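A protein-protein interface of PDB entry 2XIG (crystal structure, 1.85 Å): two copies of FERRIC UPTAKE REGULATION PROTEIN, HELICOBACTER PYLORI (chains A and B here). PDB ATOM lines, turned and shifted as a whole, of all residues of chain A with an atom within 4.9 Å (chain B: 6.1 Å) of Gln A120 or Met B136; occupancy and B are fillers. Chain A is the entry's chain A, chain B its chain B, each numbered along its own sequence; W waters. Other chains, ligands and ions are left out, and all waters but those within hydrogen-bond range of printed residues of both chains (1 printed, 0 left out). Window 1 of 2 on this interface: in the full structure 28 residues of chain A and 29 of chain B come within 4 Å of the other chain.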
ATOM      1  N   ILE A 116      24.420   7.289  16.303  1.00  0.00           N
ATOM      2  CA  ILE A 116      25.124   8.338  17.027  1.00  0.00           C
ATOM      3  C   ILE A 116      24.835   9.703  16.410  1.00  0.00           C
ATOM      4  O   ILE A 116      24.563  10.672  17.118  1.00  0.00           O
ATOM      5  CB  ILE A 116      26.642   8.093  17.038  1.00  0.00           C
ATOM      6  CG1 ILE A 116      26.967   6.880  17.913  1.00  0.00           C
ATOM      7  CG2 ILE A 116      27.384   9.339  17.513  1.00  0.00           C
ATOM      8  CD1 ILE A 116      28.430   6.707  18.212  1.00  0.00           C
ATOM      9  N   GLU A 117      24.905   9.779  15.087  1.00  0.00           N
ATOM     10  CA  GLU A 117      24.634  11.037  14.398  1.00  0.00           C
ATOM     11  C   GLU A 117      23.212  11.512  14.682  1.00  0.00           C
ATOM     12  O   GLU A 117      22.977  12.699  14.899  1.00  0.00           O
ATOM     13  CB  GLU A 117      24.847  10.890  12.893  1.00  0.00           C
ATOM     14  CG  GLU A 117      26.202  10.332  12.492  1.00  0.00           C
ATOM     15  CD  GLU A 117      27.348  11.288  12.761  1.00  0.00           C
ATOM     16  OE1 GLU A 117      27.165  12.518  12.608  1.00  0.00           O
ATOM     17  OE2 GLU A 117      28.437  10.798  13.114  1.00  0.00           O
ATOM     18  N   ASN A 118      22.259  10.584  14.677  1.00  0.00           N
ATOM     19  CA  ASN A 118      20.875  10.947  14.955  1.00  0.00           C
ATOM     20  C   ASN A 118      20.733  11.455  16.375  1.00  0.00           C
ATOM     21  O   ASN A 118      20.102  12.484  16.618  1.00  0.00           O
ATOM     22  CB  ASN A 118      19.931   9.761  14.735  1.00  0.00           C
ATOM     23  CG  ASN A 118      18.502  10.066  15.163  1.00  0.00           C
ATOM     24  OD1 ASN A 118      17.954  11.121  14.839  1.00  0.00           O
ATOM     25  ND2 ASN A 118      17.892   9.136  15.887  1.00  0.00           N
ATOM     26  N   ARG A 119      21.339  10.736  17.316  1.00  0.00           N
ATOM     27  CA  ARG A 119      21.193  11.071  18.723  1.00  0.00           C
ATOM     28  C   ARG A 119      21.810  12.427  19.044  1.00  0.00           C
ATOM     29  O   ARG A 119      21.301  13.151  19.897  1.00  0.00           O
ATOM     30  CB  ARG A 119      21.791   9.974  19.610  1.00  0.00           C
ATOM     31  CG  ARG A 119      21.669  10.252  21.106  1.00  0.00           C
ATOM     32  CD  ARG A 119      20.218  10.467  21.508  1.00  0.00           C
ATOM     33  NE  ARG A 119      20.089  10.894  22.899  1.00  0.00           N
ATOM     34  CZ  ARG A 119      18.943  11.241  23.476  1.00  0.00           C
ATOM     35  NH1 ARG A 119      17.810  11.220  22.782  1.00  0.00           N
ATOM     36  NH2 ARG A 119      18.931  11.612  24.748  1.00  0.00           N
ATOM     37  N   GLN A 120      22.904  12.768  18.366  1.00  0.00           N
ATOM     38  CA  GLN A 120      23.525  14.081  18.535  1.00  0.00           C
ATOM     39  C   GLN A 120      22.527  15.178  18.173  1.00  0.00           C
ATOM     40  O   GLN A 120      22.516  16.252  18.770  1.00  0.00           O
ATOM     41  CB  GLN A 120      24.770  14.215  17.652  1.00  0.00           C
ATOM     42  CG  GLN A 120      25.947  13.347  18.078  1.00  0.00           C
ATOM     43  CD  GLN A 120      27.092  13.385  17.079  1.00  0.00           C
ATOM     44  OE1 GLN A 120      26.944  13.874  15.957  1.00  0.00           O
ATOM     45  NE2 GLN A 120      28.239  12.862  17.481  1.00  0.00           N
ATOM     46  N   ASN A 121      21.691  14.904  17.182  1.00  0.00           N
ATOM     47  CA  ASN A 121      20.694  15.876  16.760  1.00  0.00           C
ATOM     48  C   ASN A 121      19.557  16.007  17.768  1.00  0.00           C
ATOM     49  O   ASN A 121      19.089  17.114  18.043  1.00  0.00           O
ATOM     50  CB  ASN A 121      20.187  15.553  15.354  1.00  0.00           C
ATOM     51  CG  ASN A 121      21.159  15.996  14.278  1.00  0.00           C
ATOM     52  OD1 ASN A 121      21.389  17.192  14.091  1.00  0.00           O
ATOM     53  ND2 ASN A 121      21.737  15.035  13.566  1.00  0.00           N
ATOM     54  N   GLU A 122      19.138  14.881  18.342  1.00  0.00           N
ATOM     55  CA  GLU A 122      18.108  14.889  19.379  1.00  0.00           C
ATOM     56  C   GLU A 122      18.581  15.647  20.619  1.00  0.00           C
ATOM     57  O   GLU A 122      17.811  16.366  21.257  1.00  0.00           O
ATOM     58  CB  GLU A 122      17.717  13.460  19.769  1.00  0.00           C
ATOM     59  CG  GLU A 122      17.124  12.630  18.643  1.00  0.00           C
ATOM     60  CD  GLU A 122      16.568  11.296  19.122  1.00  0.00           C
ATOM     61  OE1 GLU A 122      17.270  10.578  19.871  1.00  0.00           O
ATOM     62  OE2 GLU A 122      15.425  10.963  18.741  1.00  0.00           O
ATOM     63  N   VAL A 123      19.853  15.474  20.961  1.00  0.00           N
ATOM     64  CA  VAL A 123      20.419  16.090  22.159  1.00  0.00           C
ATOM     65  C   VAL A 123      20.472  17.612  22.049  1.00  0.00           C
ATOM     66  O   VAL A 123      20.136  18.325  22.995  1.00  0.00           O
ATOM     67  CB  VAL A 123      21.825  15.528  22.457  1.00  0.00           C
ATOM     68  CG1 VAL A 123      22.552  16.384  23.479  1.00  0.00           C
ATOM     69  CG2 VAL A 123      21.721  14.084  22.926  1.00  0.00           C
ATOM     70  N   VAL A 124      20.889  18.110  20.891  1.00  0.00           N
ATOM     71  CA  VAL A 124      20.991  19.549  20.692  1.00  0.00           C
ATOM     72  C   VAL A 124      19.610  20.211  20.657  1.00  0.00           C
ATOM     73  O   VAL A 124      19.454  21.359  21.066  1.00  0.00           O
ATOM     74  CB  VAL A 124      21.803  19.891  19.434  1.00  0.00           C
ATOM     75  CG1 VAL A 124      21.826  21.386  19.207  1.00  0.00           C
ATOM     76  CG2 VAL A 124      23.221  19.367  19.581  1.00  0.00           C
ATOM     77  N   LEU A 131      22.682  22.441  15.367  1.00  0.00           N
ATOM     78  CA  LEU A 131      23.949  21.741  15.164  1.00  0.00           C
ATOM     79  C   LEU A 131      24.601  22.120  13.844  1.00  0.00           C
ATOM     80  O   LEU A 131      24.046  21.878  12.769  1.00  0.00           O
ATOM     81  CB  LEU A 131      23.750  20.229  15.218  1.00  0.00           C
ATOM     82  CG  LEU A 131      25.043  19.414  15.117  1.00  0.00           C
ATOM     83  CD1 LEU A 131      26.016  19.802  16.230  1.00  0.00           C
ATOM     84  CD2 LEU A 131      24.740  17.923  15.164  1.00  0.00           C
ATOM     85  N   HIS A 134      30.441  18.765  14.334  1.00  0.00           N
ATOM     86  CA  HIS A 134      30.951  18.153  15.549  1.00  0.00           C
ATOM     87  C   HIS A 134      32.314  17.542  15.311  1.00  0.00           C
ATOM     88  O   HIS A 134      32.774  17.416  14.178  1.00  0.00           O
ATOM     89  CB  HIS A 134      29.971  17.104  16.082  1.00  0.00           C
ATOM     90  CG  HIS A 134      29.730  15.978  15.134  1.00  0.00           C
ATOM     91  ND1 HIS A 134      28.855  16.075  14.072  1.00  0.00           N
ATOM     92  CD2 HIS A 134      30.261  14.735  15.073  1.00  0.00           C
ATOM     93  CE1 HIS A 134      28.854  14.938  13.401  1.00  0.00           C
ATOM     94  NE2 HIS A 134      29.693  14.106  13.992  1.00  0.00           N
ATOM     95  N   ASP A 135      32.969  17.168  16.402  1.00  0.00           N
ATOM     96  CA  ASP A 135      34.242  16.506  16.298  1.00  0.00           C
ATOM     97  C   ASP A 135      34.248  15.442  17.382  1.00  0.00           C
ATOM     98  O   ASP A 135      34.030  15.743  18.549  1.00  0.00           O
ATOM     99  CB  ASP A 135      35.376  17.511  16.471  1.00  0.00           C
ATOM    100  CG  ASP A 135      36.737  16.883  16.270  1.00  0.00           C
ATOM    101  OD1 ASP A 135      37.153  16.078  17.128  1.00  0.00           O
ATOM    102  OD2 ASP A 135      37.395  17.192  15.255  1.00  0.00           O
ATOM    103  N   MET A 136      34.432  14.194  16.974  1.00  0.00           N
ATOM    104  CA  MET A 136      34.313  13.071  17.892  1.00  0.00           C
ATOM    105  C   MET A 136      35.512  12.168  17.706  1.00  0.00           C
ATOM    106  O   MET A 136      35.763  11.684  16.604  1.00  0.00           O
ATOM    107  CB  MET A 136      33.009  12.303  17.638  1.00  0.00           C
ATOM    108  CG  MET A 136      32.895  10.970  18.381  1.00  0.00           C
ATOM    109  SD  MET A 136      31.292  10.179  18.080  1.00  0.00           S
ATOM    110  CE  MET A 136      31.562   8.551  18.743  1.00  0.00           C
ATOM    111  N   HIS B  97      32.098  15.039  31.240  1.00  0.00           N
ATOM    112  CA  HIS B  97      31.059  15.618  30.416  1.00  0.00           C
ATOM    113  C   HIS B  97      31.646  16.007  29.077  1.00  0.00           C
ATOM    114  O   HIS B  97      32.864  16.133  28.931  1.00  0.00           O
ATOM    115  CB  HIS B  97      30.443  16.841  31.096  1.00  0.00           C
ATOM    116  CG  HIS B  97      31.426  17.932  31.374  1.00  0.00           C
ATOM    117  ND1 HIS B  97      32.292  17.900  32.448  1.00  0.00           N
ATOM    118  CD2 HIS B  97      31.693  19.083  30.712  1.00  0.00           C
ATOM    119  CE1 HIS B  97      33.043  18.986  32.439  1.00  0.00           C
ATOM    120  NE2 HIS B  97      32.694  19.723  31.399  1.00  0.00           N
ATOM    121  N   ASP B  98      30.765  16.178  28.101  1.00  0.00           N
ATOM    122  CA  ASP B  98      31.161  16.642  26.783  1.00  0.00           C
ATOM    123  C   ASP B  98      30.648  18.065  26.596  1.00  0.00           C
ATOM    124  O   ASP B  98      30.034  18.620  27.505  1.00  0.00           O
ATOM    125  CB  ASP B  98      30.604  15.698  25.728  1.00  0.00           C
ATOM    126  CG  ASP B  98      31.005  14.266  25.985  1.00  0.00           C
ATOM    127  OD1 ASP B  98      30.112  13.456  26.308  1.00  0.00           O
ATOM    128  OD2 ASP B  98      32.218  13.970  25.900  1.00  0.00           O
ATOM    129  N   HIS B  99      30.906  18.665  25.438  1.00  0.00           N
ATOM    130  CA  HIS B  99      30.630  20.088  25.287  1.00  0.00           C
ATOM    131  C   HIS B  99      29.877  20.452  24.037  1.00  0.00           C
ATOM    132  O   HIS B  99      30.258  20.059  22.942  1.00  0.00           O
ATOM    133  CB  HIS B  99      31.924  20.878  25.249  1.00  0.00           C
ATOM    134  CG  HIS B  99      32.787  20.658  26.438  1.00  0.00           C
ATOM    135  ND1 HIS B  99      33.758  19.684  26.471  1.00  0.00           N
ATOM    136  CD2 HIS B  99      32.820  21.273  27.643  1.00  0.00           C
ATOM    137  CE1 HIS B  99      34.356  19.709  27.649  1.00  0.00           C
ATOM    138  NE2 HIS B  99      33.811  20.669  28.371  1.00  0.00           N
ATOM    139  N   ILE B 100      28.831  21.242  24.234  1.00  0.00           N
ATOM    140  CA  ILE B 100      28.162  21.963  23.163  1.00  0.00           C
ATOM    141  C   ILE B 100      28.748  23.375  23.167  1.00  0.00           C
ATOM    142  O   ILE B 100      28.794  24.026  24.205  1.00  0.00           O
ATOM    143  CB  ILE B 100      26.643  21.979  23.415  1.00  0.00           C
ATOM    144  CG1 ILE B 100      26.061  20.599  23.100  1.00  0.00           C
ATOM    145  CG2 ILE B 100      25.952  23.073  22.600  1.00  0.00           C
ATOM    146  CD1 ILE B 100      24.670  20.371  23.632  1.00  0.00           C
ATOM    147  N   PHE B 111      27.155  18.565  28.726  1.00  0.00           N
ATOM    148  CA  PHE B 111      26.176  17.493  28.638  1.00  0.00           C
ATOM    149  C   PHE B 111      26.852  16.142  28.815  1.00  0.00           C
ATOM    150  O   PHE B 111      28.049  15.994  28.577  1.00  0.00           O
ATOM    151  CB  PHE B 111      25.406  17.544  27.306  1.00  0.00           C
ATOM    152  CG  PHE B 111      26.212  17.087  26.116  1.00  0.00           C
ATOM    153  CD1 PHE B 111      26.124  15.784  25.664  1.00  0.00           C
ATOM    154  CD2 PHE B 111      27.081  17.953  25.477  1.00  0.00           C
ATOM    155  CE1 PHE B 111      26.871  15.356  24.584  1.00  0.00           C
ATOM    156  CE2 PHE B 111      27.835  17.532  24.395  1.00  0.00           C
ATOM    157  CZ  PHE B 111      27.724  16.229  23.944  1.00  0.00           C
ATOM    158  N   ILE B 116      24.526   8.275  23.927  1.00  0.00           N
ATOM    159  CA  ILE B 116      25.777   8.524  23.218  1.00  0.00           C
ATOM    160  C   ILE B 116      26.940   7.803  23.913  1.00  0.00           C
ATOM    161  O   ILE B 116      27.720   7.110  23.260  1.00  0.00           O
ATOM    162  CB  ILE B 116      26.074  10.030  23.107  1.00  0.00           C
ATOM    163  CG1 ILE B 116      25.110  10.683  22.110  1.00  0.00           C
ATOM    164  CG2 ILE B 116      27.529  10.261  22.702  1.00  0.00           C
ATOM    165  CD1 ILE B 116      25.233  12.184  22.024  1.00  0.00           C
ATOM    166  N   GLN B 120      28.977   4.747  21.994  1.00  0.00           N
ATOM    167  CA  GLN B 120      30.397   4.901  21.703  1.00  0.00           C
ATOM    168  C   GLN B 120      31.155   3.621  22.036  1.00  0.00           C
ATOM    169  O   GLN B 120      32.048   3.206  21.302  1.00  0.00           O
ATOM    170  CB  GLN B 120      30.984   6.077  22.489  1.00  0.00           C
ATOM    171  CG  GLN B 120      30.604   7.442  21.916  1.00  0.00           C
ATOM    172  CD  GLN B 120      31.059   8.603  22.798  1.00  0.00           C
ATOM    173  OE1 GLN B 120      31.294   8.435  23.994  1.00  0.00           O
ATOM    174  NE2 GLN B 120      31.172   9.787  22.207  1.00  0.00           N
ATOM    175  N   HIS B 134      37.433   9.750  25.448  1.00  0.00           N
ATOM    176  CA  HIS B 134      36.969  10.298  24.187  1.00  0.00           C
ATOM    177  C   HIS B 134      36.892  11.805  24.271  1.00  0.00           C
ATOM    178  O   HIS B 134      36.886  12.373  25.356  1.00  0.00           O
ATOM    179  CB  HIS B 134      35.615   9.704  23.814  1.00  0.00           C
ATOM    180  CG  HIS B 134      34.543   9.966  24.820  1.00  0.00           C
ATOM    181  ND1 HIS B 134      34.347   9.161  25.921  1.00  0.00           N
ATOM    182  CD2 HIS B 134      33.596  10.929  24.884  1.00  0.00           C
ATOM    183  CE1 HIS B 134      33.330   9.624  26.626  1.00  0.00           C
ATOM    184  NE2 HIS B 134      32.851  10.693  26.013  1.00  0.00           N
ATOM    185  N   ASP B 135      36.834  12.439  23.105  1.00  0.00           N
ATOM    186  CA  ASP B 135      36.835  13.877  23.016  1.00  0.00           C
ATOM    187  C   ASP B 135      35.710  14.157  22.048  1.00  0.00           C
ATOM    188  O   ASP B 135      35.742  13.717  20.908  1.00  0.00           O
ATOM    189  CB  ASP B 135      38.173  14.362  22.464  1.00  0.00           C
ATOM    190  CG  ASP B 135      38.241  15.870  22.322  1.00  0.00           C
ATOM    191  OD1 ASP B 135      37.313  16.569  22.793  1.00  0.00           O
ATOM    192  OD2 ASP B 135      39.231  16.357  21.734  1.00  0.00           O
ATOM    193  N   MET B 136      34.695  14.857  22.519  1.00  0.00           N
ATOM    194  CA  MET B 136      33.486  14.996  21.744  1.00  0.00           C
ATOM    195  C   MET B 136      32.956  16.386  21.960  1.00  0.00           C
ATOM    196  O   MET B 136      32.692  16.793  23.089  1.00  0.00           O
ATOM    197  CB  MET B 136      32.484  13.956  22.230  1.00  0.00           C
ATOM    198  CG  MET B 136      31.381  13.641  21.270  1.00  0.00           C
ATOM    199  SD  MET B 136      29.980  14.718  21.523  1.00  0.00           S
ATOM    200  CE  MET B 136      28.658  13.554  21.212  1.00  0.00           C
ATOM    201  N   LYS B 137      32.822  17.142  20.882  1.00  0.00           N
ATOM    202  CA  LYS B 137      32.217  18.444  21.014  1.00  0.00           C
ATOM    203  C   LYS B 137      31.315  18.728  19.841  1.00  0.00           C
ATOM    204  O   LYS B 137      31.572  18.299  18.727  1.00  0.00           O
ATOM    205  CB  LYS B 137      33.264  19.544  21.207  1.00  0.00           C
ATOM    206  CG  LYS B 137      34.359  19.587  20.173  1.00  0.00           C
ATOM    207  CD  LYS B 137      35.664  20.041  20.816  1.00  0.00           C
ATOM    208  CE  LYS B 137      36.810  19.973  19.827  1.00  0.00           C
ATOM    209  NZ  LYS B 137      38.067  19.515  20.482  1.00  0.00           N
ATOM    210  N   MET B 138      30.232  19.425  20.128  1.00  0.00           N
ATOM    211  CA  MET B 138      29.268  19.781  19.107  1.00  0.00           C
ATOM    212  C   MET B 138      29.220  21.282  19.002  1.00  0.00           C
ATOM    213  O   MET B 138      29.020  21.974  19.997  1.00  0.00           O
ATOM    214  CB  MET B 138      27.898  19.217  19.471  1.00  0.00           C
ATOM    215  CG  MET B 138      27.903  17.703  19.546  1.00  0.00           C
ATOM    216  SD  MET B 138      26.252  16.998  19.541  1.00  0.00           S
ATOM    217  CE  MET B 138      25.685  17.429  21.185  1.00  0.00           C
HETATM  218  O   HOH W   1      36.770  16.517  19.807  1.00  0.00           O
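The backbone carbonyl oxygen of Lys B137 is in hydrogen-bond range of the backbone NH of Asp A135, at 2.9 Å.
NH1 of Arg A119 lies within salt-bridge range of OE1 of Glu A122 (3.0 Å).
ND1 of His A134 lies close to OE1 of Gln A120 (3.5 Å).
The backbone NH (N) of His B99 sits at hydrogen-bond distance from the backbone carbonyl oxygen (O) of Met B136, at 3.5 Å.
The backbone NH of Met B138 is in hydrogen-bond range of the backbone carbonyl oxygen of His B99 (2.9 Å).
A ring nitrogen (NE2) of His B134 lies close to the side-chain amide oxygen of Gln B120, at 3.4 Å.
The side-chain carboxylate (OD2) of Asp B135 is in salt-bridge range of the side-chain amino group (NZ) of Lys B137, 3.6 Å away.
Among the printed residues, pairs that only touch across the chains: His A134 with Lys B137, Asp A135 with Met B136, Met A136 with Asp B135, Met A136 with Gln B120, Val A124 with Met B138, Asp A135 with Asp B135, Arg A119 with Ile B116, Gln A120 with Met B138, Leu A131 with Met B138 and Gln A120 with Met B136.
Gln A120 touches just these residues of chain B: Met B136 (3.8 Å) and Met B138 (3.7 Å).
Of chain A, only Gln A120 and Asp A135 come within 4 Å of Met B136.
Of the printed residues of chain B, Val A124 touches Met B138 (3.5 Å).
Of the printed residues of chain A, Ile B116 touches Arg A119.
Of the printed residues of chain B, Arg A119 touches Ile B116 (3.6 Å).
Of the printed residues of chain A, Asp B135 touches Asp A135 (3.5 Å) and Met A136 (3.4 Å).
Ile B100 touches none of the printed residues of chain A.
The nearest residue of chain B that does not touch Gln A120 is Ile B116 (4.2 Å).
The nearest residue of chain A that does not touch Met B136 is Met A136 (4.2 Å).
Hydrophobic or aromatic side chains of chain A that line the printed part of chain B: Val A124, Leu A131, His A134 and Met A136.
Hydrophobic or aromatic side chains of chain B that line the printed part of chain A: Ile B116, Met B136 and Met B138.
Among the printed residues, no Asp or Glu carboxylate lies within 4 Å of a Lys or Arg side-chain nitrogen of the other chain.
Gln A120 touches Met B136, and with the chains exchanged Met A136 touches Gln B120.
Asp A135 touches its own counterpart, Asp B135.
Asp A135 touches Met B136, and with the chains exchanged Met A136 touches Asp B135.
5 positions are printed for both chains.
Water W1 lies within hydrogen-bond range of the side-chain carboxylate of Asp A135 (2.7 Å), the side-chain carboxylate of Asp B135 (3.0 Å) and the side-chain amino group of Lys B137 (3.3 Å).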
